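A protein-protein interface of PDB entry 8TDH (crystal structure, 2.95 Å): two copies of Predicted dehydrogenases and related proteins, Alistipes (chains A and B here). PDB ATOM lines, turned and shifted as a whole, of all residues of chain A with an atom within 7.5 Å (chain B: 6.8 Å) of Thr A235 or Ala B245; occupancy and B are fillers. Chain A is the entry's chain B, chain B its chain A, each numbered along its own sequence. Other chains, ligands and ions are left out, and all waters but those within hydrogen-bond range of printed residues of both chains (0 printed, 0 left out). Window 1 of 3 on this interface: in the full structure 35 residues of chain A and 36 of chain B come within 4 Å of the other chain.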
ATOM      1  N   GLY A 159     -10.114 -15.855  -1.599  1.00  0.00           N
ATOM      2  CA  GLY A 159     -10.312 -16.649  -0.399  1.00  0.00           C
ATOM      3  C   GLY A 159     -11.608 -17.449  -0.457  1.00  0.00           C
ATOM      4  O   GLY A 159     -12.173 -17.693   0.602  1.00  0.00           O
ATOM      5  N   SER A 233       4.765 -14.890   1.957  1.00  0.00           N
ATOM      6  CA  SER A 233       3.821 -15.214   3.003  1.00  0.00           C
ATOM      7  C   SER A 233       2.508 -14.554   2.594  1.00  0.00           C
ATOM      8  O   SER A 233       2.531 -13.742   1.679  1.00  0.00           O
ATOM      9  CB  SER A 233       4.320 -14.763   4.362  1.00  0.00           C
ATOM     10  OG  SER A 233       4.417 -13.345   4.414  1.00  0.00           O
ATOM     11  N   SER A 234       1.379 -14.933   3.229  1.00  0.00           N
ATOM     12  CA  SER A 234       0.075 -14.439   2.821  1.00  0.00           C
ATOM     13  C   SER A 234      -0.970 -14.610   3.912  1.00  0.00           C
ATOM     14  O   SER A 234      -0.706 -15.224   4.934  1.00  0.00           O
ATOM     15  CB  SER A 234      -0.370 -15.127   1.584  1.00  0.00           C
ATOM     16  OG  SER A 234      -0.838 -16.456   1.839  1.00  0.00           O
ATOM     17  N   THR A 235      -2.178 -14.062   3.691  1.00  0.00           N
ATOM     18  CA  THR A 235      -3.320 -14.375   4.546  1.00  0.00           C
ATOM     19  C   THR A 235      -3.752 -15.807   4.257  1.00  0.00           C
ATOM     20  O   THR A 235      -3.194 -16.444   3.372  1.00  0.00           O
ATOM     21  CB  THR A 235      -4.461 -13.386   4.333  1.00  0.00           C
ATOM     22  OG1 THR A 235      -4.640 -13.373   2.932  1.00  0.00           O
ATOM     23  CG2 THR A 235      -4.127 -11.979   4.765  1.00  0.00           C
ATOM     24  N   LEU A 236      -4.776 -16.285   4.974  1.00  0.00           N
ATOM     25  CA  LEU A 236      -5.290 -17.642   4.827  1.00  0.00           C
ATOM     26  C   LEU A 236      -5.061 -18.155   3.416  1.00  0.00           C
ATOM     27  O   LEU A 236      -5.580 -17.556   2.472  1.00  0.00           O
ATOM     28  CB  LEU A 236      -6.779 -17.676   5.129  1.00  0.00           C
ATOM     29  CG  LEU A 236      -7.421 -19.062   5.060  1.00  0.00           C
ATOM     30  CD1 LEU A 236      -6.717 -19.950   6.096  1.00  0.00           C
ATOM     31  CD2 LEU A 236      -8.943 -18.966   5.281  1.00  0.00           C
ATOM     32  N   LEU A 237      -4.331 -19.270   3.311  1.00  0.00           N
ATOM     33  CA  LEU A 237      -3.977 -19.827   2.011  1.00  0.00           C
ATOM     34  C   LEU A 237      -4.779 -21.092   1.693  1.00  0.00           C
ATOM     35  O   LEU A 237      -4.589 -22.139   2.319  1.00  0.00           O
ATOM     36  CB  LEU A 237      -2.491 -20.152   1.942  1.00  0.00           C
ATOM     37  CG  LEU A 237      -2.117 -20.978   0.710  1.00  0.00           C
ATOM     38  CD1 LEU A 237      -2.149 -20.166  -0.578  1.00  0.00           C
ATOM     39  CD2 LEU A 237      -0.757 -21.543   0.930  1.00  0.00           C
ATOM     40  N   LEU A 238      -5.572 -21.021   0.624  1.00  0.00           N
ATOM     41  CA  LEU A 238      -6.484 -22.098   0.292  1.00  0.00           C
ATOM     42  C   LEU A 238      -5.960 -22.893  -0.883  1.00  0.00           C
ATOM     43  O   LEU A 238      -4.953 -22.513  -1.479  1.00  0.00           O
ATOM     44  CB  LEU A 238      -7.833 -21.474   0.008  1.00  0.00           C
ATOM     45  CG  LEU A 238      -8.434 -20.703   1.179  1.00  0.00           C
ATOM     46  CD1 LEU A 238      -9.725 -20.059   0.750  1.00  0.00           C
ATOM     47  CD2 LEU A 238      -8.671 -21.674   2.300  1.00  0.00           C
ATOM     48  N   ALA A 242      -6.713 -17.943  -4.519  1.00  0.00           N
ATOM     49  CA  ALA A 242      -5.661 -17.045  -4.086  1.00  0.00           C
ATOM     50  C   ALA A 242      -6.095 -16.234  -2.858  1.00  0.00           C
ATOM     51  O   ALA A 242      -7.277 -16.106  -2.570  1.00  0.00           O
ATOM     52  CB  ALA A 242      -5.299 -16.152  -5.248  1.00  0.00           C
ATOM     53  N   PRO A 243      -5.162 -15.646  -2.067  1.00  0.00           N
ATOM     54  CA  PRO A 243      -5.509 -15.041  -0.786  1.00  0.00           C
ATOM     55  C   PRO A 243      -5.775 -13.553  -0.857  1.00  0.00           C
ATOM     56  O   PRO A 243      -5.461 -12.923  -1.846  1.00  0.00           O
ATOM     57  CB  PRO A 243      -4.215 -15.342   0.011  1.00  0.00           C
ATOM     58  CG  PRO A 243      -3.220 -15.969  -0.959  1.00  0.00           C
ATOM     59  CD  PRO A 243      -3.713 -15.553  -2.317  1.00  0.00           C
ATOM     60  N   MET A 244      -6.270 -12.997   0.244  1.00  0.00           N
ATOM     61  CA  MET A 244      -6.698 -11.609   0.358  1.00  0.00           C
ATOM     62  C   MET A 244      -5.542 -10.646   0.135  1.00  0.00           C
ATOM     63  O   MET A 244      -5.726  -9.585  -0.435  1.00  0.00           O
ATOM     64  CB  MET A 244      -7.325 -11.397   1.755  1.00  0.00           C
ATOM     65  CG  MET A 244      -7.658  -9.973   2.170  1.00  0.00           C
ATOM     66  SD  MET A 244      -9.320  -9.519   2.726  1.00  0.00           S
ATOM     67  CE  MET A 244      -9.234 -10.233   4.367  1.00  0.00           C
ATOM     68  N   ALA A 245      -4.372 -11.032   0.629  1.00  0.00           N
ATOM     69  CA  ALA A 245      -3.177 -10.192   0.716  1.00  0.00           C
ATOM     70  C   ALA A 245      -1.921 -11.063   0.799  1.00  0.00           C
ATOM     71  O   ALA A 245      -1.903 -12.045   1.556  1.00  0.00           O
ATOM     72  CB  ALA A 245      -3.264  -9.336   1.962  1.00  0.00           C
ATOM     73  N   GLN A 246      -0.871 -10.715   0.041  1.00  0.00           N
ATOM     74  CA  GLN A 246       0.381 -11.457   0.091  1.00  0.00           C
ATOM     75  C   GLN A 246       1.541 -10.469   0.192  1.00  0.00           C
ATOM     76  O   GLN A 246       1.353  -9.308  -0.123  1.00  0.00           O
ATOM     77  CB  GLN A 246       0.376 -12.464  -1.068  1.00  0.00           C
ATOM     78  CG  GLN A 246       0.417 -11.896  -2.485  1.00  0.00           C
ATOM     79  CD  GLN A 246      -0.403 -12.748  -3.447  1.00  0.00           C
ATOM     80  OE1 GLN A 246      -0.314 -13.998  -3.511  1.00  0.00           O
ATOM     81  NE2 GLN A 246      -1.249 -12.074  -4.220  1.00  0.00           N
ATOM     82  N   THR A 247       2.697 -10.925   0.725  1.00  0.00           N
ATOM     83  CA  THR A 247       4.015 -10.288   0.584  1.00  0.00           C
ATOM     84  C   THR A 247       4.985 -11.277  -0.055  1.00  0.00           C
ATOM     85  O   THR A 247       5.112 -12.377   0.433  1.00  0.00           O
ATOM     86  CB  THR A 247       4.632  -9.820   1.918  1.00  0.00           C
ATOM     87  OG1 THR A 247       4.906 -10.943   2.764  1.00  0.00           O
ATOM     88  CG2 THR A 247       3.761  -8.797   2.641  1.00  0.00           C
ATOM     89  N   ASP A 272       0.688  -6.518  -1.542  1.00  0.00           N
ATOM     90  CA  ASP A 272      -0.613  -6.210  -2.092  1.00  0.00           C
ATOM     91  C   ASP A 272      -1.706  -6.495  -1.083  1.00  0.00           C
ATOM     92  O   ASP A 272      -1.450  -7.107  -0.041  1.00  0.00           O
ATOM     93  CB  ASP A 272      -0.855  -6.959  -3.388  1.00  0.00           C
ATOM     94  CG  ASP A 272      -1.015  -8.454  -3.287  1.00  0.00           C
ATOM     95  OD1 ASP A 272      -1.782  -8.889  -2.410  1.00  0.00           O
ATOM     96  OD2 ASP A 272      -0.419  -9.184  -4.109  1.00  0.00           O
ATOM     97  N   GLY A 273      -2.931  -6.082  -1.441  1.00  0.00           N
ATOM     98  CA  GLY A 273      -4.128  -6.410  -0.683  1.00  0.00           C
ATOM     99  C   GLY A 273      -4.355  -5.440   0.460  1.00  0.00           C
ATOM    100  O   GLY A 273      -5.112  -5.700   1.365  1.00  0.00           O
ATOM    101  N   GLY A 274      -3.681  -4.301   0.374  1.00  0.00           N
ATOM    102  CA  GLY A 274      -3.776  -3.247   1.370  1.00  0.00           C
ATOM    103  C   GLY A 274      -2.450  -3.007   2.074  1.00  0.00           C
ATOM    104  O   GLY A 274      -2.202  -1.898   2.545  1.00  0.00           O
ATOM    105  N   LEU A 275      -1.596  -4.034   2.100  1.00  0.00           N
ATOM    106  CA  LEU A 275      -0.302  -3.921   2.752  1.00  0.00           C
ATOM    107  C   LEU A 275       0.550  -2.978   1.917  1.00  0.00           C
ATOM    108  O   LEU A 275       0.431  -3.014   0.695  1.00  0.00           O
ATOM    109  CB  LEU A 275       0.376  -5.276   2.858  1.00  0.00           C
ATOM    110  CG  LEU A 275      -0.454  -6.360   3.542  1.00  0.00           C
ATOM    111  CD1 LEU A 275       0.281  -7.672   3.389  1.00  0.00           C
ATOM    112  CD2 LEU A 275      -0.702  -6.021   4.981  1.00  0.00           C
ATOM    113  N   VAL A 374       4.205 -18.088  -2.777  1.00  0.00           N
ATOM    114  CA  VAL A 374       3.095 -17.978  -1.852  1.00  0.00           C
ATOM    115  C   VAL A 374       2.586 -19.370  -1.489  1.00  0.00           C
ATOM    116  O   VAL A 374       2.246 -19.593  -0.334  1.00  0.00           O
ATOM    117  CB  VAL A 374       1.988 -17.083  -2.434  1.00  0.00           C
ATOM    118  CG1 VAL A 374       0.694 -17.259  -1.687  1.00  0.00           C
ATOM    119  CG2 VAL A 374       2.408 -15.610  -2.461  1.00  0.00           C
ATOM    120  N   GLN A 377       4.741 -21.716   0.814  1.00  0.00           N
ATOM    121  CA  GLN A 377       5.135 -20.991   1.993  1.00  0.00           C
ATOM    122  C   GLN A 377       5.269 -21.859   3.229  1.00  0.00           C
ATOM    123  O   GLN A 377       5.891 -21.460   4.189  1.00  0.00           O
ATOM    124  CB  GLN A 377       4.182 -19.843   2.235  1.00  0.00           C
ATOM    125  CG  GLN A 377       2.810 -20.197   2.774  1.00  0.00           C
ATOM    126  CD  GLN A 377       2.058 -18.925   3.091  1.00  0.00           C
ATOM    127  OE1 GLN A 377       2.255 -18.276   4.122  1.00  0.00           O
ATOM    128  NE2 GLN A 377       1.261 -18.476   2.147  1.00  0.00           N
ATOM    129  N   ARG B 153      -2.399 -15.322  14.463  1.00  0.00           N
ATOM    130  CA  ARG B 153      -3.681 -14.702  14.737  1.00  0.00           C
ATOM    131  C   ARG B 153      -3.903 -13.484  13.845  1.00  0.00           C
ATOM    132  O   ARG B 153      -2.954 -12.950  13.297  1.00  0.00           O
ATOM    133  CB  ARG B 153      -3.706 -14.236  16.194  1.00  0.00           C
ATOM    134  CG  ARG B 153      -4.206 -15.242  17.218  1.00  0.00           C
ATOM    135  CD  ARG B 153      -3.465 -16.518  17.145  1.00  0.00           C
ATOM    136  NE  ARG B 153      -3.768 -17.312  18.332  1.00  0.00           N
ATOM    137  CZ  ARG B 153      -3.216 -18.464  18.625  1.00  0.00           C
ATOM    138  NH1 ARG B 153      -2.203 -18.921  17.900  1.00  0.00           N
ATOM    139  NH2 ARG B 153      -3.656 -19.080  19.703  1.00  0.00           N
ATOM    140  N   PRO B 154      -5.136 -12.990  13.606  1.00  0.00           N
ATOM    141  CA  PRO B 154      -6.373 -13.646  14.054  1.00  0.00           C
ATOM    142  C   PRO B 154      -6.673 -15.018  13.432  1.00  0.00           C
ATOM    143  O   PRO B 154      -6.399 -15.230  12.257  1.00  0.00           O
ATOM    144  CB  PRO B 154      -7.414 -12.593  13.624  1.00  0.00           C
ATOM    145  CG  PRO B 154      -6.822 -11.945  12.364  1.00  0.00           C
ATOM    146  CD  PRO B 154      -5.387 -11.771  12.809  1.00  0.00           C
ATOM    147  N   GLN B 158     -12.378 -11.663  11.154  1.00  0.00           N
ATOM    148  CA  GLN B 158     -12.552 -10.239  11.368  1.00  0.00           C
ATOM    149  C   GLN B 158     -13.071  -9.713  10.046  1.00  0.00           C
ATOM    150  O   GLN B 158     -13.474 -10.522   9.230  1.00  0.00           O
ATOM    151  CB  GLN B 158     -11.269  -9.607  11.916  1.00  0.00           C
ATOM    152  CG  GLN B 158     -10.734 -10.378  13.107  1.00  0.00           C
ATOM    153  CD  GLN B 158      -9.859  -9.553  14.002  1.00  0.00           C
ATOM    154  OE1 GLN B 158     -10.061  -9.444  15.225  1.00  0.00           O
ATOM    155  NE2 GLN B 158      -8.857  -8.995  13.363  1.00  0.00           N
ATOM    156  N   SER B 233      -0.097  -0.438   7.925  1.00  0.00           N
ATOM    157  CA  SER B 233      -0.983  -0.665   6.795  1.00  0.00           C
ATOM    158  C   SER B 233      -1.748  -1.958   7.077  1.00  0.00           C
ATOM    159  O   SER B 233      -1.358  -2.669   8.016  1.00  0.00           O
ATOM    160  CB  SER B 233      -0.172  -0.705   5.533  1.00  0.00           C
ATOM    161  OG  SER B 233       0.693  -1.839   5.530  1.00  0.00           O
ATOM    162  N   SER B 234      -2.827  -2.212   6.324  1.00  0.00           N
ATOM    163  CA  SER B 234      -3.616  -3.412   6.594  1.00  0.00           C
ATOM    164  C   SER B 234      -4.446  -3.853   5.390  1.00  0.00           C
ATOM    165  O   SER B 234      -4.488  -3.129   4.407  1.00  0.00           O
ATOM    166  CB  SER B 234      -4.491  -3.212   7.808  1.00  0.00           C
ATOM    167  OG  SER B 234      -5.582  -2.372   7.497  1.00  0.00           O
ATOM    168  N   THR B 235      -5.085  -5.021   5.472  1.00  0.00           N
ATOM    169  CA  THR B 235      -6.102  -5.385   4.505  1.00  0.00           C
ATOM    170  C   THR B 235      -7.305  -4.466   4.721  1.00  0.00           C
ATOM    171  O   THR B 235      -7.350  -3.729   5.693  1.00  0.00           O
ATOM    172  CB  THR B 235      -6.539  -6.850   4.644  1.00  0.00           C
ATOM    173  OG1 THR B 235      -6.989  -7.068   5.968  1.00  0.00           O
ATOM    174  CG2 THR B 235      -5.457  -7.870   4.359  1.00  0.00           C
ATOM    175  N   LEU B 236      -8.279  -4.515   3.809  1.00  0.00           N
ATOM    176  CA  LEU B 236      -9.436  -3.636   3.842  1.00  0.00           C
ATOM    177  C   LEU B 236      -9.765  -3.296   5.282  1.00  0.00           C
ATOM    178  O   LEU B 236      -9.992  -4.201   6.092  1.00  0.00           O
ATOM    179  CB  LEU B 236     -10.626  -4.344   3.198  1.00  0.00           C
ATOM    180  CG  LEU B 236     -11.939  -3.563   3.155  1.00  0.00           C
ATOM    181  CD1 LEU B 236     -11.786  -2.210   2.436  1.00  0.00           C
ATOM    182  CD2 LEU B 236     -13.013  -4.381   2.459  1.00  0.00           C
ATOM    183  N   ALA B 242     -11.945  -4.936  13.102  1.00  0.00           N
ATOM    184  CA  ALA B 242     -10.520  -5.011  12.820  1.00  0.00           C
ATOM    185  C   ALA B 242     -10.264  -5.811  11.540  1.00  0.00           C
ATOM    186  O   ALA B 242     -11.103  -6.588  11.111  1.00  0.00           O
ATOM    187  CB  ALA B 242      -9.813  -5.566  14.040  1.00  0.00           C
ATOM    188  N   PRO B 243      -9.106  -5.675  10.876  1.00  0.00           N
ATOM    189  CA  PRO B 243      -8.913  -6.287   9.568  1.00  0.00           C
ATOM    190  C   PRO B 243      -8.225  -7.628   9.670  1.00  0.00           C
ATOM    191  O   PRO B 243      -7.623  -7.953  10.698  1.00  0.00           O
ATOM    192  CB  PRO B 243      -7.997  -5.250   8.891  1.00  0.00           C
ATOM    193  CG  PRO B 243      -7.596  -4.232   9.998  1.00  0.00           C
ATOM    194  CD  PRO B 243      -7.941  -4.889  11.310  1.00  0.00           C
ATOM    195  N   MET B 244      -8.237  -8.340   8.556  1.00  0.00           N
ATOM    196  CA  MET B 244      -7.789  -9.726   8.498  1.00  0.00           C
ATOM    197  C   MET B 244      -6.307  -9.846   8.777  1.00  0.00           C
ATOM    198  O   MET B 244      -5.895 -10.817   9.398  1.00  0.00           O
ATOM    199  CB  MET B 244      -8.053 -10.347   7.129  1.00  0.00           C
ATOM    200  CG  MET B 244      -8.123 -11.870   7.168  1.00  0.00           C
ATOM    201  SD  MET B 244      -8.207 -12.616   5.517  1.00  0.00           S
ATOM    202  CE  MET B 244      -8.803 -14.331   5.579  1.00  0.00           C
ATOM    203  N   ALA B 245      -5.543  -8.850   8.313  1.00  0.00           N
ATOM    204  CA  ALA B 245      -4.093  -8.813   8.455  1.00  0.00           C
ATOM    205  C   ALA B 245      -3.531  -7.383   8.523  1.00  0.00           C
ATOM    206  O   ALA B 245      -3.904  -6.575   7.677  1.00  0.00           O
ATOM    207  CB  ALA B 245      -3.514  -9.569   7.276  1.00  0.00           C
ATOM    208  N   GLN B 246      -2.594  -7.099   9.447  1.00  0.00           N
ATOM    209  CA  GLN B 246      -1.948  -5.796   9.499  1.00  0.00           C
ATOM    210  C   GLN B 246      -0.433  -5.934   9.576  1.00  0.00           C
ATOM    211  O   GLN B 246       0.037  -6.980   9.958  1.00  0.00           O
ATOM    212  CB  GLN B 246      -2.635  -5.013  10.619  1.00  0.00           C
ATOM    213  CG  GLN B 246      -2.398  -5.488  12.053  1.00  0.00           C
ATOM    214  CD  GLN B 246      -3.614  -5.226  12.923  1.00  0.00           C
ATOM    215  OE1 GLN B 246      -4.210  -4.132  12.975  1.00  0.00           O
ATOM    216  NE2 GLN B 246      -4.046  -6.300  13.588  1.00  0.00           N
ATOM    217  N   THR B 247       0.302  -4.896   9.108  1.00  0.00           N
ATOM    218  CA  THR B 247       1.731  -4.655   9.408  1.00  0.00           C
ATOM    219  C   THR B 247       1.888  -3.306  10.095  1.00  0.00           C
ATOM    220  O   THR B 247       1.403  -2.334   9.590  1.00  0.00           O
ATOM    221  CB  THR B 247       2.649  -4.654   8.179  1.00  0.00           C
ATOM    222  OG1 THR B 247       2.263  -3.614   7.286  1.00  0.00           O
ATOM    223  CG2 THR B 247       2.627  -5.980   7.439  1.00  0.00           C
ATOM    224  N   ASP B 272       0.896  -9.735  11.265  1.00  0.00           N
ATOM    225  CA  ASP B 272      -0.051 -10.770  11.672  1.00  0.00           C
ATOM    226  C   ASP B 272      -1.010 -11.129  10.546  1.00  0.00           C
ATOM    227  O   ASP B 272      -1.073 -10.463   9.531  1.00  0.00           O
ATOM    228  CB  ASP B 272      -0.816 -10.370  12.922  1.00  0.00           C
ATOM    229  CG  ASP B 272      -1.798  -9.208  12.755  1.00  0.00           C
ATOM    230  OD1 ASP B 272      -2.600  -9.248  11.779  1.00  0.00           O
ATOM    231  OD2 ASP B 272      -1.793  -8.262  13.600  1.00  0.00           O
ATOM    232  N   GLY B 273      -1.777 -12.178  10.774  1.00  0.00           N
ATOM    233  CA  GLY B 273      -2.840 -12.577   9.871  1.00  0.00           C
ATOM    234  C   GLY B 273      -2.305 -13.506   8.787  1.00  0.00           C
ATOM    235  O   GLY B 273      -2.940 -13.711   7.765  1.00  0.00           O
ATOM    236  N   GLY B 274      -1.123 -14.063   9.028  1.00  0.00           N
ATOM    237  CA  GLY B 274      -0.482 -14.926   8.059  1.00  0.00           C
ATOM    238  C   GLY B 274       0.859 -14.345   7.637  1.00  0.00           C
ATOM    239  O   GLY B 274       1.792 -15.100   7.294  1.00  0.00           O
ATOM    240  N   LEU B 275       0.950 -13.012   7.680  1.00  0.00           N
ATOM    241  CA  LEU B 275       2.095 -12.308   7.133  1.00  0.00           C
ATOM    242  C   LEU B 275       3.276 -12.587   8.040  1.00  0.00           C
ATOM    243  O   LEU B 275       3.084 -12.633   9.244  1.00  0.00           O
ATOM    244  CB  LEU B 275       1.824 -10.814   7.042  1.00  0.00           C
ATOM    245  CG  LEU B 275       0.525 -10.395   6.359  1.00  0.00           C
ATOM    246  CD1 LEU B 275       0.478  -8.898   6.376  1.00  0.00           C
ATOM    247  CD2 LEU B 275       0.438 -10.918   4.971  1.00  0.00           C
ATOM    248  N   VAL B 374      -2.930   1.713  12.632  1.00  0.00           N
ATOM    249  CA  VAL B 374      -3.630   1.036  11.569  1.00  0.00           C
ATOM    250  C   VAL B 374      -4.843   1.856  11.142  1.00  0.00           C
ATOM    251  O   VAL B 374      -5.133   1.882   9.958  1.00  0.00           O
ATOM    252  CB  VAL B 374      -4.039  -0.376  12.010  1.00  0.00           C
ATOM    253  CG1 VAL B 374      -5.116  -0.974  11.131  1.00  0.00           C
ATOM    254  CG2 VAL B 374      -2.856  -1.297  11.992  1.00  0.00           C
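O of Gly B274 lies close to O of Ser A234. O of Gly A274 sits close to O of Ser B234, at 3.2 Å.
The backbone carbonyl oxygen (O) of Arg B153 sits at hydrogen-bond distance from the backbone NH (N) of Gly B273, at 2.9 Å. OG1 of Thr B235 is in hydrogen-bond range of N of Met B244 (3.1 Å). The backbone carbonyl oxygen (O) of Ala B245 is in hydrogen-bond range of the backbone NH (N) of Thr B235, 2.9 Å away. The side-chain hydroxyl of Thr A247 sits at hydrogen-bond distance from the side-chain hydroxyl of Ser A233 (3.0 Å). OG of Ser A234 lies within hydrogen-bond range of NE2 of Gln A377 (2.9 Å). OG1 of Thr A235 sits at hydrogen-bond distance from N of Met A244.
Gly B274 touches Ser A233 (O to CB, 3.9 Å). Gly B273 touches Ser A234 (O to O, 3.9 Å). Ser A234 touches Leu B275. CG2 of Thr A235 touches CB of Ala B245, at 3.5 Å. Thr B235 touches Met A244. Thr B235 touches Ala A245 (CG2 to CB, 3.6 Å). Gly A273 touches Thr B235 (O to CA, 3.3 Å). CB of Ser B233 touches O of Gly A274 (3.8 Å). Leu A275 touches Ser B234 (N to O, 3.8 Å). Leu B275 touches Leu A275 (CD1 to CD1, 3.2 Å).
Of the printed residues of chain B, Thr A235 touches Ala B245 and Gly B273. Of the printed residues of chain B, Gly A273 touches Thr B235. Printed residues of chain B within 4 Å of Leu A236: Met B244 (3.9 Å). Of the printed residues of chain A, Ser B234 touches Gly A274 (3.1 Å) and Leu A275 (3.8 Å). Of the printed residues of chain B, Ser A233 touches Gly B274 and Leu B275. Printed residues of chain B within 4 Å of Leu A275: Ser B233, Ser B234 and Leu B275.
Of the 18 printed residues of chain B, 8 touch a printed residue of chain A. Hydrophobic or aromatic side chains of chain A that line the printed part of chain B: Leu A236, Met A244, Ala A245 and Leu A275. Among the printed residues, no Asp or Glu carboxylate lies within 4 Å of a Lys or Arg side-chain nitrogen of the other chain.
Ser A234 touches Gly B274, and with the chains exchanged Gly A274 touches Ser B234. Thr A235 touches Ala B245, and with the chains exchanged Ala A245 touches Thr B235. Met A244 touches Thr B235, but with the chains exchanged Thr A235 does not touch Met B244 (4.003 Å). Leu B275 touches its own counterpart, Leu A275.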
